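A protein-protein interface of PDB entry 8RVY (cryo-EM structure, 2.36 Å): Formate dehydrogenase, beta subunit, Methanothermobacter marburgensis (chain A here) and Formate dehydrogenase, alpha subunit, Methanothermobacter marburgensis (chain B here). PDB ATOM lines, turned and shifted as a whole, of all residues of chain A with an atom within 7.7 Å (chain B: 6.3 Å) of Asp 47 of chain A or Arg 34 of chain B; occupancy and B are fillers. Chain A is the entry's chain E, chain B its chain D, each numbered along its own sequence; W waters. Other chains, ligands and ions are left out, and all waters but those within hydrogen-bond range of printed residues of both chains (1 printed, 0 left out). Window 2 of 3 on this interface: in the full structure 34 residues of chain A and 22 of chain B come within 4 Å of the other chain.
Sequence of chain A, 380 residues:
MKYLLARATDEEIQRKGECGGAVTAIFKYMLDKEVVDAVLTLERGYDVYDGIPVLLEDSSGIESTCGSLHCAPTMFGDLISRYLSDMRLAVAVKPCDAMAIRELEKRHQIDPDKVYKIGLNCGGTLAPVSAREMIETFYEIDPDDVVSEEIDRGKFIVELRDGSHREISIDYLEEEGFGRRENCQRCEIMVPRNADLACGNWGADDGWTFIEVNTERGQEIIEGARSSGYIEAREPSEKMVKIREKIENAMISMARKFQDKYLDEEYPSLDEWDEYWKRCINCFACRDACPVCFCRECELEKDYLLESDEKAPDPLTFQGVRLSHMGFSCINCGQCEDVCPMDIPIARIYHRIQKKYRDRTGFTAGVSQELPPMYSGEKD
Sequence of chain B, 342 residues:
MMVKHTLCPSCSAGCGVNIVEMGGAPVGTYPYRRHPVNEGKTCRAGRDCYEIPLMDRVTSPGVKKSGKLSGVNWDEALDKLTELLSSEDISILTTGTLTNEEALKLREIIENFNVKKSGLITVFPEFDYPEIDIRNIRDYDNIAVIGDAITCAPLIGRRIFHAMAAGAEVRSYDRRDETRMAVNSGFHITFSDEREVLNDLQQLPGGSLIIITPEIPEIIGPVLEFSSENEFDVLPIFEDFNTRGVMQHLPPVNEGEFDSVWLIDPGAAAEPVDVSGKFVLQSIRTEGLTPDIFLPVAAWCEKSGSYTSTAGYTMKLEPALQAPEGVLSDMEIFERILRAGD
O of Glu 43 of chain A is in hydrogen-bond range of N of Ile 52 of chain A, at 2.9 Å. The side-chain carboxylate (OD1) of Asp 47 of chain A lies close to the backbone NH (N) of Tyr 49 of chain A, 3.2 Å away. The side-chain carboxylate of Asp 47 of chain A sits at hydrogen-bond distance from the backbone NH of Asp 50 of chain A (3.1 Å). The side-chain hydroxyl (OH) of Tyr 49 of chain A is in hydrogen-bond range of the backbone carbonyl oxygen (O) of Pro 143 of chain A, at 3.2 Å. The guanidinium group (NH2) of Arg 132 of chain A lies within salt-bridge range of the side-chain carboxylate (OD1) of Asp 144 of chain A (2.8 Å). The backbone NH (N) of Gly 40 of chain B sits at hydrogen-bond distance from the backbone carbonyl oxygen (O) of Tyr 32 of chain B (3.0 Å).
Water W1 bridges O of Arg 33 of chain B (2.7 Å) and N of Val 129 of chain A (3.2 Å).
Among the printed residues, merely in contact across the chains: Tyr 46 of chain A with Arg 34 of chain B (3.2 Å), Tyr 49 of chain A with Arg 34 of chain B (3.6 Å), Asp 50 of chain A with Arg 34 of chain B (3.5 Å), Ile 52 of chain A with His 5 of chain B (3.5 Å), Pro 128 of chain A with Arg 33 of chain B (3.97 Å), Val 129 of chain A with Arg 33 of chain B (3.8 Å), Val 129 of chain A with Arg 34 of chain B (3.8 Å), Val 129 of chain A with His 35 of chain B (3.7 Å) and Val 129 of chain A with Glu 39 of chain B (3.7 Å).
Of the 21 printed residues of chain A, 8 touch a printed residue of chain B. Hydrophobic or aromatic side chains of chain A that line the printed part of chain B: Tyr 46, Tyr 49, Ile 52, Pro 128 and Val 129. Printed residues of chain B that touch a printed residue of chain A: His 5, Tyr 32, Arg 33, Arg 34, His 35 and Glu 39. Along chain B the printed residues that touch a printed residue of chain A span positions 5 to 39.
The side-chain hydroxyl (OH) of Tyr 46 of chain A is in hydrogen-bond range of the side-chain hydroxyl (OH) of Tyr 32 of chain B, at 3.5 Å. The guanidinium group (NH2) of Arg 34 of chain B is in salt-bridge range of the side-chain carboxylate (OD2) of Asp 47 of chain A (3.0 Å). The side-chain carboxylate (OD2) of Asp 50 of chain A sits at hydrogen-bond distance from a ring nitrogen (NE2) of His 5 of chain B (2.9 Å). The guanidinium group (NH1) of Arg 132 of chain A sits close to the guanidinium group (NH2) of Arg 34 of chain B.
Asp 47 of chain A touches just one residue of chain B: Arg 34. Arg 34 of chain B touches just these residues of chain A: Tyr 46 (3.2 Å), Asp 47 (3.0 Å), Tyr 49 (3.6 Å), Asp 50 (3.5 Å), Val 129 (3.8 Å) and Arg 132 (3.3 Å). Of the printed residues of chain A, His 35 of chain B touches Val 129 (3.7 Å). Of the printed residues of chain A, Tyr 32 of chain B touches Tyr 46. Of the printed residues of chain A, Glu 39 of chain B touches Val 129 (3.7 Å). Printed residues of chain B within 4 Å of Ile 52 of chain A: His 5 (3.5 Å). Gly 51 of chain A touches none of the printed residues of chain B. The nearest printed residue of chain B that does not touch Asp 47 of chain A is His 5 of chain B (7.7 Å).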
ATOM      1  N   GLU A  43      25.052  17.664  27.704  1.00  0.00           N
ATOM      2  CA  GLU A  43      25.781  18.923  27.728  1.00  0.00           C
ATOM      3  C   GLU A  43      25.064  19.887  26.801  1.00  0.00           C
ATOM      4  O   GLU A  43      24.775  19.538  25.656  1.00  0.00           O
ATOM      5  CB  GLU A  43      27.233  18.726  27.288  1.00  0.00           C
ATOM      6  CG  GLU A  43      28.105  19.947  27.470  1.00  0.00           C
ATOM      7  CD  GLU A  43      29.551  19.670  27.136  1.00  0.00           C
ATOM      8  OE1 GLU A  43      29.864  19.509  25.939  1.00  0.00           O
ATOM      9  OE2 GLU A  43      30.375  19.608  28.070  1.00  0.00           O
ATOM     10  N   ARG A  44      24.759  21.080  27.295  1.00  0.00           N
ATOM     11  CA  ARG A  44      24.058  22.042  26.460  1.00  0.00           C
ATOM     12  C   ARG A  44      24.925  22.426  25.269  1.00  0.00           C
ATOM     13  O   ARG A  44      26.154  22.481  25.357  1.00  0.00           O
ATOM     14  CB  ARG A  44      23.675  23.282  27.266  1.00  0.00           C
ATOM     15  CG  ARG A  44      24.845  24.161  27.655  1.00  0.00           C
ATOM     16  CD  ARG A  44      24.473  25.071  28.804  1.00  0.00           C
ATOM     17  NE  ARG A  44      24.360  24.330  30.056  1.00  0.00           N
ATOM     18  CZ  ARG A  44      23.462  24.571  31.002  1.00  0.00           C
ATOM     19  NH1 ARG A  44      22.582  25.553  30.893  1.00  0.00           N
ATOM     20  NH2 ARG A  44      23.447  23.803  32.088  1.00  0.00           N
ATOM     21  N   GLY A  45      24.270  22.695  24.147  1.00  0.00           N
ATOM     22  CA  GLY A  45      24.967  23.055  22.931  1.00  0.00           C
ATOM     23  C   GLY A  45      25.147  24.553  22.837  1.00  0.00           C
ATOM     24  O   GLY A  45      25.902  25.136  23.619  1.00  0.00           O
ATOM     25  N   TYR A  46      24.469  25.191  21.887  1.00  0.00           N
ATOM     26  CA  TYR A  46      24.541  26.637  21.741  1.00  0.00           C
ATOM     27  C   TYR A  46      23.411  27.365  22.459  1.00  0.00           C
ATOM     28  O   TYR A  46      23.325  28.591  22.359  1.00  0.00           O
ATOM     29  CB  TYR A  46      24.555  27.024  20.256  1.00  0.00           C
ATOM     30  CG  TYR A  46      23.405  26.486  19.435  1.00  0.00           C
ATOM     31  CD1 TYR A  46      22.231  27.210  19.293  1.00  0.00           C
ATOM     32  CD2 TYR A  46      23.503  25.265  18.784  1.00  0.00           C
ATOM     33  CE1 TYR A  46      21.184  26.728  18.538  1.00  0.00           C
ATOM     34  CE2 TYR A  46      22.458  24.773  18.026  1.00  0.00           C
ATOM     35  CZ  TYR A  46      21.303  25.510  17.906  1.00  0.00           C
ATOM     36  OH  TYR A  46      20.262  25.026  17.152  1.00  0.00           O
ATOM     37  N   ASP A  47      22.547  26.651  23.177  1.00  0.00           N
ATOM     38  CA  ASP A  47      21.544  27.282  24.027  1.00  0.00           C
ATOM     39  C   ASP A  47      20.956  26.215  24.940  1.00  0.00           C
ATOM     40  O   ASP A  47      21.225  25.021  24.784  1.00  0.00           O
ATOM     41  CB  ASP A  47      20.454  27.986  23.209  1.00  0.00           C
ATOM     42  CG  ASP A  47      19.821  27.087  22.162  1.00  0.00           C
ATOM     43  OD1 ASP A  47      19.775  25.861  22.365  1.00  0.00           O
ATOM     44  OD2 ASP A  47      19.356  27.617  21.133  1.00  0.00           O
ATOM     45  N   VAL A  48      20.155  26.664  25.909  1.00  0.00           N
ATOM     46  CA  VAL A  48      19.581  25.750  26.893  1.00  0.00           C
ATOM     47  C   VAL A  48      18.659  24.734  26.241  1.00  0.00           C
ATOM     48  O   VAL A  48      18.361  23.697  26.841  1.00  0.00           O
ATOM     49  CB  VAL A  48      18.819  26.521  27.993  1.00  0.00           C
ATOM     50  CG1 VAL A  48      19.792  27.107  29.002  1.00  0.00           C
ATOM     51  CG2 VAL A  48      17.931  27.602  27.389  1.00  0.00           C
ATOM     52  N   TYR A  49      18.194  25.007  25.028  1.00  0.00           N
ATOM     53  CA  TYR A  49      17.288  24.121  24.316  1.00  0.00           C
ATOM     54  C   TYR A  49      18.007  23.048  23.514  1.00  0.00           C
ATOM     55  O   TYR A  49      17.343  22.243  22.855  1.00  0.00           O
ATOM     56  CB  TYR A  49      16.399  24.936  23.377  1.00  0.00           C
ATOM     57  CG  TYR A  49      15.724  26.111  24.031  1.00  0.00           C
ATOM     58  CD1 TYR A  49      14.541  25.953  24.732  1.00  0.00           C
ATOM     59  CD2 TYR A  49      16.266  27.383  23.938  1.00  0.00           C
ATOM     60  CE1 TYR A  49      13.917  27.026  25.324  1.00  0.00           C
ATOM     61  CE2 TYR A  49      15.652  28.462  24.528  1.00  0.00           C
ATOM     62  CZ  TYR A  49      14.478  28.279  25.219  1.00  0.00           C
ATOM     63  OH  TYR A  49      13.861  29.354  25.811  1.00  0.00           O
ATOM     64  N   ASP A  50      19.335  23.011  23.550  1.00  0.00           N
ATOM     65  CA  ASP A  50      20.135  22.113  22.722  1.00  0.00           C
ATOM     66  C   ASP A  50      21.042  21.286  23.630  1.00  0.00           C
ATOM     67  O   ASP A  50      22.189  21.656  23.883  1.00  0.00           O
ATOM     68  CB  ASP A  50      20.941  22.913  21.710  1.00  0.00           C
ATOM     69  CG  ASP A  50      21.687  22.035  20.735  1.00  0.00           C
ATOM     70  OD1 ASP A  50      21.142  20.989  20.331  1.00  0.00           O
ATOM     71  OD2 ASP A  50      22.825  22.394  20.371  1.00  0.00           O
ATOM     72  N   GLY A  51      20.525  20.156  24.111  1.00  0.00           N
ATOM     73  CA  GLY A  51      21.281  19.257  24.947  1.00  0.00           C
ATOM     74  C   GLY A  51      21.738  18.052  24.153  1.00  0.00           C
ATOM     75  O   GLY A  51      20.919  17.276  23.662  1.00  0.00           O
ATOM     76  N   ILE A  52      23.052  17.900  24.035  1.00  0.00           N
ATOM     77  CA  ILE A  52      23.644  16.839  23.228  1.00  0.00           C
ATOM     78  C   ILE A  52      24.304  15.827  24.157  1.00  0.00           C
ATOM     79  O   ILE A  52      24.917  16.222  25.159  1.00  0.00           O
ATOM     80  CB  ILE A  52      24.653  17.410  22.221  1.00  0.00           C
ATOM     81  CG1 ILE A  52      24.023  18.553  21.424  1.00  0.00           C
ATOM     82  CG2 ILE A  52      25.126  16.330  21.267  1.00  0.00           C
ATOM     83  CD1 ILE A  52      24.738  19.863  21.586  1.00  0.00           C
ATOM     84  N   LEU A  69      18.481  20.144  32.187  1.00  0.00           N
ATOM     85  CA  LEU A  69      17.971  20.589  30.895  1.00  0.00           C
ATOM     86  C   LEU A  69      16.596  19.958  30.711  1.00  0.00           C
ATOM     87  O   LEU A  69      16.478  18.824  30.245  1.00  0.00           O
ATOM     88  CB  LEU A  69      18.927  20.208  29.769  1.00  0.00           C
ATOM     89  CG  LEU A  69      20.358  20.726  29.913  1.00  0.00           C
ATOM     90  CD1 LEU A  69      21.302  19.985  28.984  1.00  0.00           C
ATOM     91  CD2 LEU A  69      20.405  22.217  29.649  1.00  0.00           C
ATOM     92  N   CYS A  71      14.399  20.699  28.595  1.00  0.00           N
ATOM     93  CA  CYS A  71      14.044  20.621  27.185  1.00  0.00           C
ATOM     94  C   CYS A  71      14.925  19.633  26.429  1.00  0.00           C
ATOM     95  O   CYS A  71      15.240  19.854  25.257  1.00  0.00           O
ATOM     96  CB  CYS A  71      14.122  22.004  26.543  1.00  0.00           C
ATOM     97  SG  CYS A  71      12.961  23.203  27.232  1.00  0.00           S
ATOM     98  N   ALA A 127       9.633  19.412  24.595  1.00  0.00           N
ATOM     99  CA  ALA A 127      10.278  19.473  23.292  1.00  0.00           C
ATOM    100  C   ALA A 127      10.892  20.858  23.104  1.00  0.00           C
ATOM    101  O   ALA A 127      10.228  21.863  23.377  1.00  0.00           O
ATOM    102  CB  ALA A 127       9.275  19.171  22.184  1.00  0.00           C
ATOM    103  N   PRO A 128      12.146  20.958  22.648  1.00  0.00           N
ATOM    104  CA  PRO A 128      12.797  22.283  22.607  1.00  0.00           C
ATOM    105  C   PRO A 128      12.063  23.320  21.768  1.00  0.00           C
ATOM    106  O   PRO A 128      11.824  24.437  22.241  1.00  0.00           O
ATOM    107  CB  PRO A 128      14.185  21.971  22.035  1.00  0.00           C
ATOM    108  CG  PRO A 128      14.382  20.526  22.198  1.00  0.00           C
ATOM    109  CD  PRO A 128      13.052  19.875  22.237  1.00  0.00           C
ATOM    110  N   VAL A 129      11.718  22.993  20.523  1.00  0.00           N
ATOM    111  CA  VAL A 129      11.077  23.974  19.652  1.00  0.00           C
ATOM    112  C   VAL A 129       9.710  24.361  20.200  1.00  0.00           C
ATOM    113  O   VAL A 129       9.320  25.537  20.172  1.00  0.00           O
ATOM    114  CB  VAL A 129      10.987  23.424  18.217  1.00  0.00           C
ATOM    115  CG1 VAL A 129      10.203  24.370  17.330  1.00  0.00           C
ATOM    116  CG2 VAL A 129      12.379  23.191  17.656  1.00  0.00           C
ATOM    117  N   ARG A 132      10.287  26.778  23.037  1.00  0.00           N
ATOM    118  CA  ARG A 132      10.573  28.131  22.573  1.00  0.00           C
ATOM    119  C   ARG A 132       9.307  28.826  22.090  1.00  0.00           C
ATOM    120  O   ARG A 132       9.089  30.010  22.375  1.00  0.00           O
ATOM    121  CB  ARG A 132      11.625  28.093  21.466  1.00  0.00           C
ATOM    122  CG  ARG A 132      12.998  27.681  21.945  1.00  0.00           C
ATOM    123  CD  ARG A 132      13.958  27.465  20.791  1.00  0.00           C
ATOM    124  NE  ARG A 132      14.173  28.683  20.017  1.00  0.00           N
ATOM    125  CZ  ARG A 132      15.042  29.635  20.331  1.00  0.00           C
ATOM    126  NH1 ARG A 132      15.813  29.545  21.401  1.00  0.00           N
ATOM    127  NH2 ARG A 132      15.137  30.706  19.551  1.00  0.00           N
ATOM    128  N   PRO A 143      12.992  33.923  23.326  1.00  0.00           N
ATOM    129  CA  PRO A 143      13.472  32.678  23.945  1.00  0.00           C
ATOM    130  C   PRO A 143      14.973  32.649  24.141  1.00  0.00           C
ATOM    131  O   PRO A 143      15.456  31.991  25.071  1.00  0.00           O
ATOM    132  CB  PRO A 143      13.012  31.593  22.961  1.00  0.00           C
ATOM    133  CG  PRO A 143      11.992  32.241  22.093  1.00  0.00           C
ATOM    134  CD  PRO A 143      12.370  33.676  22.017  1.00  0.00           C
ATOM    135  N   ASP A 144      15.729  33.345  23.293  1.00  0.00           N
ATOM    136  CA  ASP A 144      17.180  33.345  23.421  1.00  0.00           C
ATOM    137  C   ASP A 144      17.643  33.986  24.721  1.00  0.00           C
ATOM    138  O   ASP A 144      18.793  33.781  25.124  1.00  0.00           O
ATOM    139  CB  ASP A 144      17.804  34.068  22.226  1.00  0.00           C
ATOM    140  CG  ASP A 144      17.336  33.505  20.895  1.00  0.00           C
ATOM    141  OD1 ASP A 144      16.998  32.305  20.840  1.00  0.00           O
ATOM    142  OD2 ASP A 144      17.309  34.261  19.903  1.00  0.00           O
ATOM    143  N   VAL A 146      16.391  33.301  27.685  1.00  0.00           N
ATOM    144  CA  VAL A 146      16.186  32.383  28.800  1.00  0.00           C
ATOM    145  C   VAL A 146      17.498  31.668  29.091  1.00  0.00           C
ATOM    146  O   VAL A 146      18.111  31.086  28.191  1.00  0.00           O
ATOM    147  CB  VAL A 146      15.067  31.380  28.490  1.00  0.00           C
ATOM    148  CG1 VAL A 146      15.006  30.304  29.561  1.00  0.00           C
ATOM    149  CG2 VAL A 146      13.735  32.099  28.369  1.00  0.00           C
ATOM    150  N   VAL A 147      17.928  31.707  30.350  1.00  0.00           N
ATOM    151  CA  VAL A 147      19.180  31.074  30.749  1.00  0.00           C
ATOM    152  C   VAL A 147      18.964  29.771  31.515  1.00  0.00           C
ATOM    153  O   VAL A 147      19.903  28.968  31.615  1.00  0.00           O
ATOM    154  CB  VAL A 147      20.039  32.052  31.582  1.00  0.00           C
ATOM    155  CG1 VAL A 147      19.658  32.002  33.048  1.00  0.00           C
ATOM    156  CG2 VAL A 147      21.512  31.741  31.412  1.00  0.00           C
ATOM    157  N   GLU A 149      15.491  26.968  33.328  1.00  0.00           N
ATOM    158  CA  GLU A 149      14.080  26.539  33.267  1.00  0.00           C
ATOM    159  C   GLU A 149      13.832  25.492  34.348  1.00  0.00           C
ATOM    160  O   GLU A 149      14.716  24.871  34.700  1.00  0.00           O
ATOM    161  CB  GLU A 149      13.866  26.039  31.839  1.00  0.00           C
ATOM    162  CG  GLU A 149      14.293  24.588  31.499  1.00  0.00           C
ATOM    163  CD  GLU A 149      15.735  24.212  31.112  1.00  0.00           C
ATOM    164  OE1 GLU A 149      16.593  24.100  31.997  1.00  0.00           O
ATOM    165  OE2 GLU A 149      15.988  23.932  29.924  1.00  0.00           O
ATOM    166  N   HIS B   5      26.197  17.845  15.388  1.00  0.00           N
ATOM    167  CA  HIS B   5      25.131  18.351  14.535  1.00  0.00           C
ATOM    168  C   HIS B   5      25.561  18.373  13.075  1.00  0.00           C
ATOM    169  O   HIS B   5      26.731  18.587  12.749  1.00  0.00           O
ATOM    170  CB  HIS B   5      24.734  19.768  14.943  1.00  0.00           C
ATOM    171  CG  HIS B   5      24.171  19.872  16.323  1.00  0.00           C
ATOM    172  ND1 HIS B   5      23.366  18.900  16.874  1.00  0.00           N
ATOM    173  CD2 HIS B   5      24.288  20.839  17.261  1.00  0.00           C
ATOM    174  CE1 HIS B   5      23.015  19.263  18.094  1.00  0.00           C
ATOM    175  NE2 HIS B   5      23.562  20.436  18.353  1.00  0.00           N
ATOM    176  N   PRO B  31      18.684  11.880  17.168  1.00  0.00           N
ATOM    177  CA  PRO B  31      17.743  12.964  16.864  1.00  0.00           C
ATOM    178  C   PRO B  31      18.317  14.336  17.177  1.00  0.00           C
ATOM    179  O   PRO B  31      18.916  14.561  18.229  1.00  0.00           O
ATOM    180  CB  PRO B  31      16.530  12.651  17.747  1.00  0.00           C
ATOM    181  CG  PRO B  31      16.863  11.433  18.519  1.00  0.00           C
ATOM    182  CD  PRO B  31      18.035  10.787  17.902  1.00  0.00           C
ATOM    183  N   TYR B  32      18.110  15.263  16.244  1.00  0.00           N
ATOM    184  CA  TYR B  32      18.466  16.668  16.417  1.00  0.00           C
ATOM    185  C   TYR B  32      17.174  17.425  16.720  1.00  0.00           C
ATOM    186  O   TYR B  32      16.578  18.068  15.860  1.00  0.00           O
ATOM    187  CB  TYR B  32      19.173  17.179  15.165  1.00  0.00           C
ATOM    188  CG  TYR B  32      19.815  18.545  15.264  1.00  0.00           C
ATOM    189  CD1 TYR B  32      19.627  19.361  16.369  1.00  0.00           C
ATOM    190  CD2 TYR B  32      20.609  19.019  14.234  1.00  0.00           C
ATOM    191  CE1 TYR B  32      20.213  20.609  16.439  1.00  0.00           C
ATOM    192  CE2 TYR B  32      21.194  20.259  14.293  1.00  0.00           C
ATOM    193  CZ  TYR B  32      20.996  21.051  15.397  1.00  0.00           C
ATOM    194  OH  TYR B  32      21.587  22.289  15.455  1.00  0.00           O
ATOM    195  N   ARG B  33      16.744  17.339  17.978  1.00  0.00           N
ATOM    196  CA  ARG B  33      15.451  17.893  18.363  1.00  0.00           C
ATOM    197  C   ARG B  33      15.431  19.411  18.269  1.00  0.00           C
ATOM    198  O   ARG B  33      14.381  19.999  17.986  1.00  0.00           O
ATOM    199  CB  ARG B  33      15.101  17.459  19.782  1.00  0.00           C
ATOM    200  CG  ARG B  33      14.537  16.062  19.882  1.00  0.00           C
ATOM    201  CD  ARG B  33      14.422  15.622  21.328  1.00  0.00           C
ATOM    202  NE  ARG B  33      13.928  14.256  21.441  1.00  0.00           N
ATOM    203  CZ  ARG B  33      14.694  13.180  21.561  1.00  0.00           C
ATOM    204  NH1 ARG B  33      16.012  13.268  21.614  1.00  0.00           N
ATOM    205  NH2 ARG B  33      14.120  11.984  21.630  1.00  0.00           N
ATOM    206  N   ARG B  34      16.569  20.059  18.514  1.00  0.00           N
ATOM    207  CA  ARG B  34      16.616  21.514  18.551  1.00  0.00           C
ATOM    208  C   ARG B  34      16.409  22.147  17.182  1.00  0.00           C
ATOM    209  O   ARG B  34      16.095  23.337  17.110  1.00  0.00           O
ATOM    210  CB  ARG B  34      17.955  21.963  19.140  1.00  0.00           C
ATOM    211  CG  ARG B  34      18.206  23.456  19.096  1.00  0.00           C
ATOM    212  CD  ARG B  34      17.164  24.226  19.876  1.00  0.00           C
ATOM    213  NE  ARG B  34      17.422  25.659  19.850  1.00  0.00           N
ATOM    214  CZ  ARG B  34      17.029  26.479  18.886  1.00  0.00           C
ATOM    215  NH1 ARG B  34      16.329  26.047  17.851  1.00  0.00           N
ATOM    216  NH2 ARG B  34      17.344  27.767  18.964  1.00  0.00           N
ATOM    217  N   HIS B  35      16.574  21.398  16.104  1.00  0.00           N
ATOM    218  CA  HIS B  35      16.469  21.990  14.778  1.00  0.00           C
ATOM    219  C   HIS B  35      15.025  22.397  14.503  1.00  0.00           C
ATOM    220  O   HIS B  35      14.108  21.613  14.763  1.00  0.00           O
ATOM    221  CB  HIS B  35      16.953  21.021  13.710  1.00  0.00           C
ATOM    222  CG  HIS B  35      17.426  21.695  12.462  1.00  0.00           C
ATOM    223  ND1 HIS B  35      16.566  22.123  11.476  1.00  0.00           N
ATOM    224  CD2 HIS B  35      18.670  22.026  12.044  1.00  0.00           C
ATOM    225  CE1 HIS B  35      17.258  22.684  10.503  1.00  0.00           C
ATOM    226  NE2 HIS B  35      18.538  22.634  10.822  1.00  0.00           N
ATOM    227  N   PRO B  36      14.778  23.598  13.968  1.00  0.00           N
ATOM    228  CA  PRO B  36      13.393  24.049  13.801  1.00  0.00           C
ATOM    229  C   PRO B  36      12.707  23.533  12.547  1.00  0.00           C
ATOM    230  O   PRO B  36      11.483  23.678  12.437  1.00  0.00           O
ATOM    231  CB  PRO B  36      13.525  25.578  13.757  1.00  0.00           C
ATOM    232  CG  PRO B  36      14.980  25.865  13.493  1.00  0.00           C
ATOM    233  CD  PRO B  36      15.733  24.583  13.436  1.00  0.00           C
ATOM    234  N   VAL B  37      13.442  22.953  11.598  1.00  0.00           N
ATOM    235  CA  VAL B  37      12.808  22.448  10.384  1.00  0.00           C
ATOM    236  C   VAL B  37      12.021  21.178  10.684  1.00  0.00           C
ATOM    237  O   VAL B  37      10.852  21.051  10.307  1.00  0.00           O
ATOM    238  CB  VAL B  37      13.859  22.213   9.284  1.00  0.00           C
ATOM    239  CG1 VAL B  37      13.285  21.359   8.163  1.00  0.00           C
ATOM    240  CG2 VAL B  37      14.354  23.531   8.737  1.00  0.00           C
ATOM    241  N   GLU B  39      12.623  19.170  13.976  1.00  0.00           N
ATOM    242  CA  GLU B  39      12.499  18.899  15.408  1.00  0.00           C
ATOM    243  C   GLU B  39      12.867  17.456  15.737  1.00  0.00           C
ATOM    244  O   GLU B  39      12.225  16.805  16.561  1.00  0.00           O
ATOM    245  CB  GLU B  39      11.089  19.222  15.904  1.00  0.00           C
ATOM    246  CG  GLU B  39      10.644  20.639  15.614  1.00  0.00           C
ATOM    247  CD  GLU B  39       9.188  20.722  15.219  1.00  0.00           C
ATOM    248  OE1 GLU B  39       8.772  19.975  14.312  1.00  0.00           O
ATOM    249  OE2 GLU B  39       8.455  21.537  15.817  1.00  0.00           O
ATOM    250  N   GLY B  40      13.919  16.955  15.095  1.00  0.00           N
ATOM    251  CA  GLY B  40      14.401  15.616  15.347  1.00  0.00           C
ATOM    252  C   GLY B  40      13.686  14.524  14.591  1.00  0.00           C
ATOM    253  O   GLY B  40      14.034  13.350  14.761  1.00  0.00           O
HETATM  254  O   HOH W   1      11.947  20.099  19.219  1.00  0.00           O
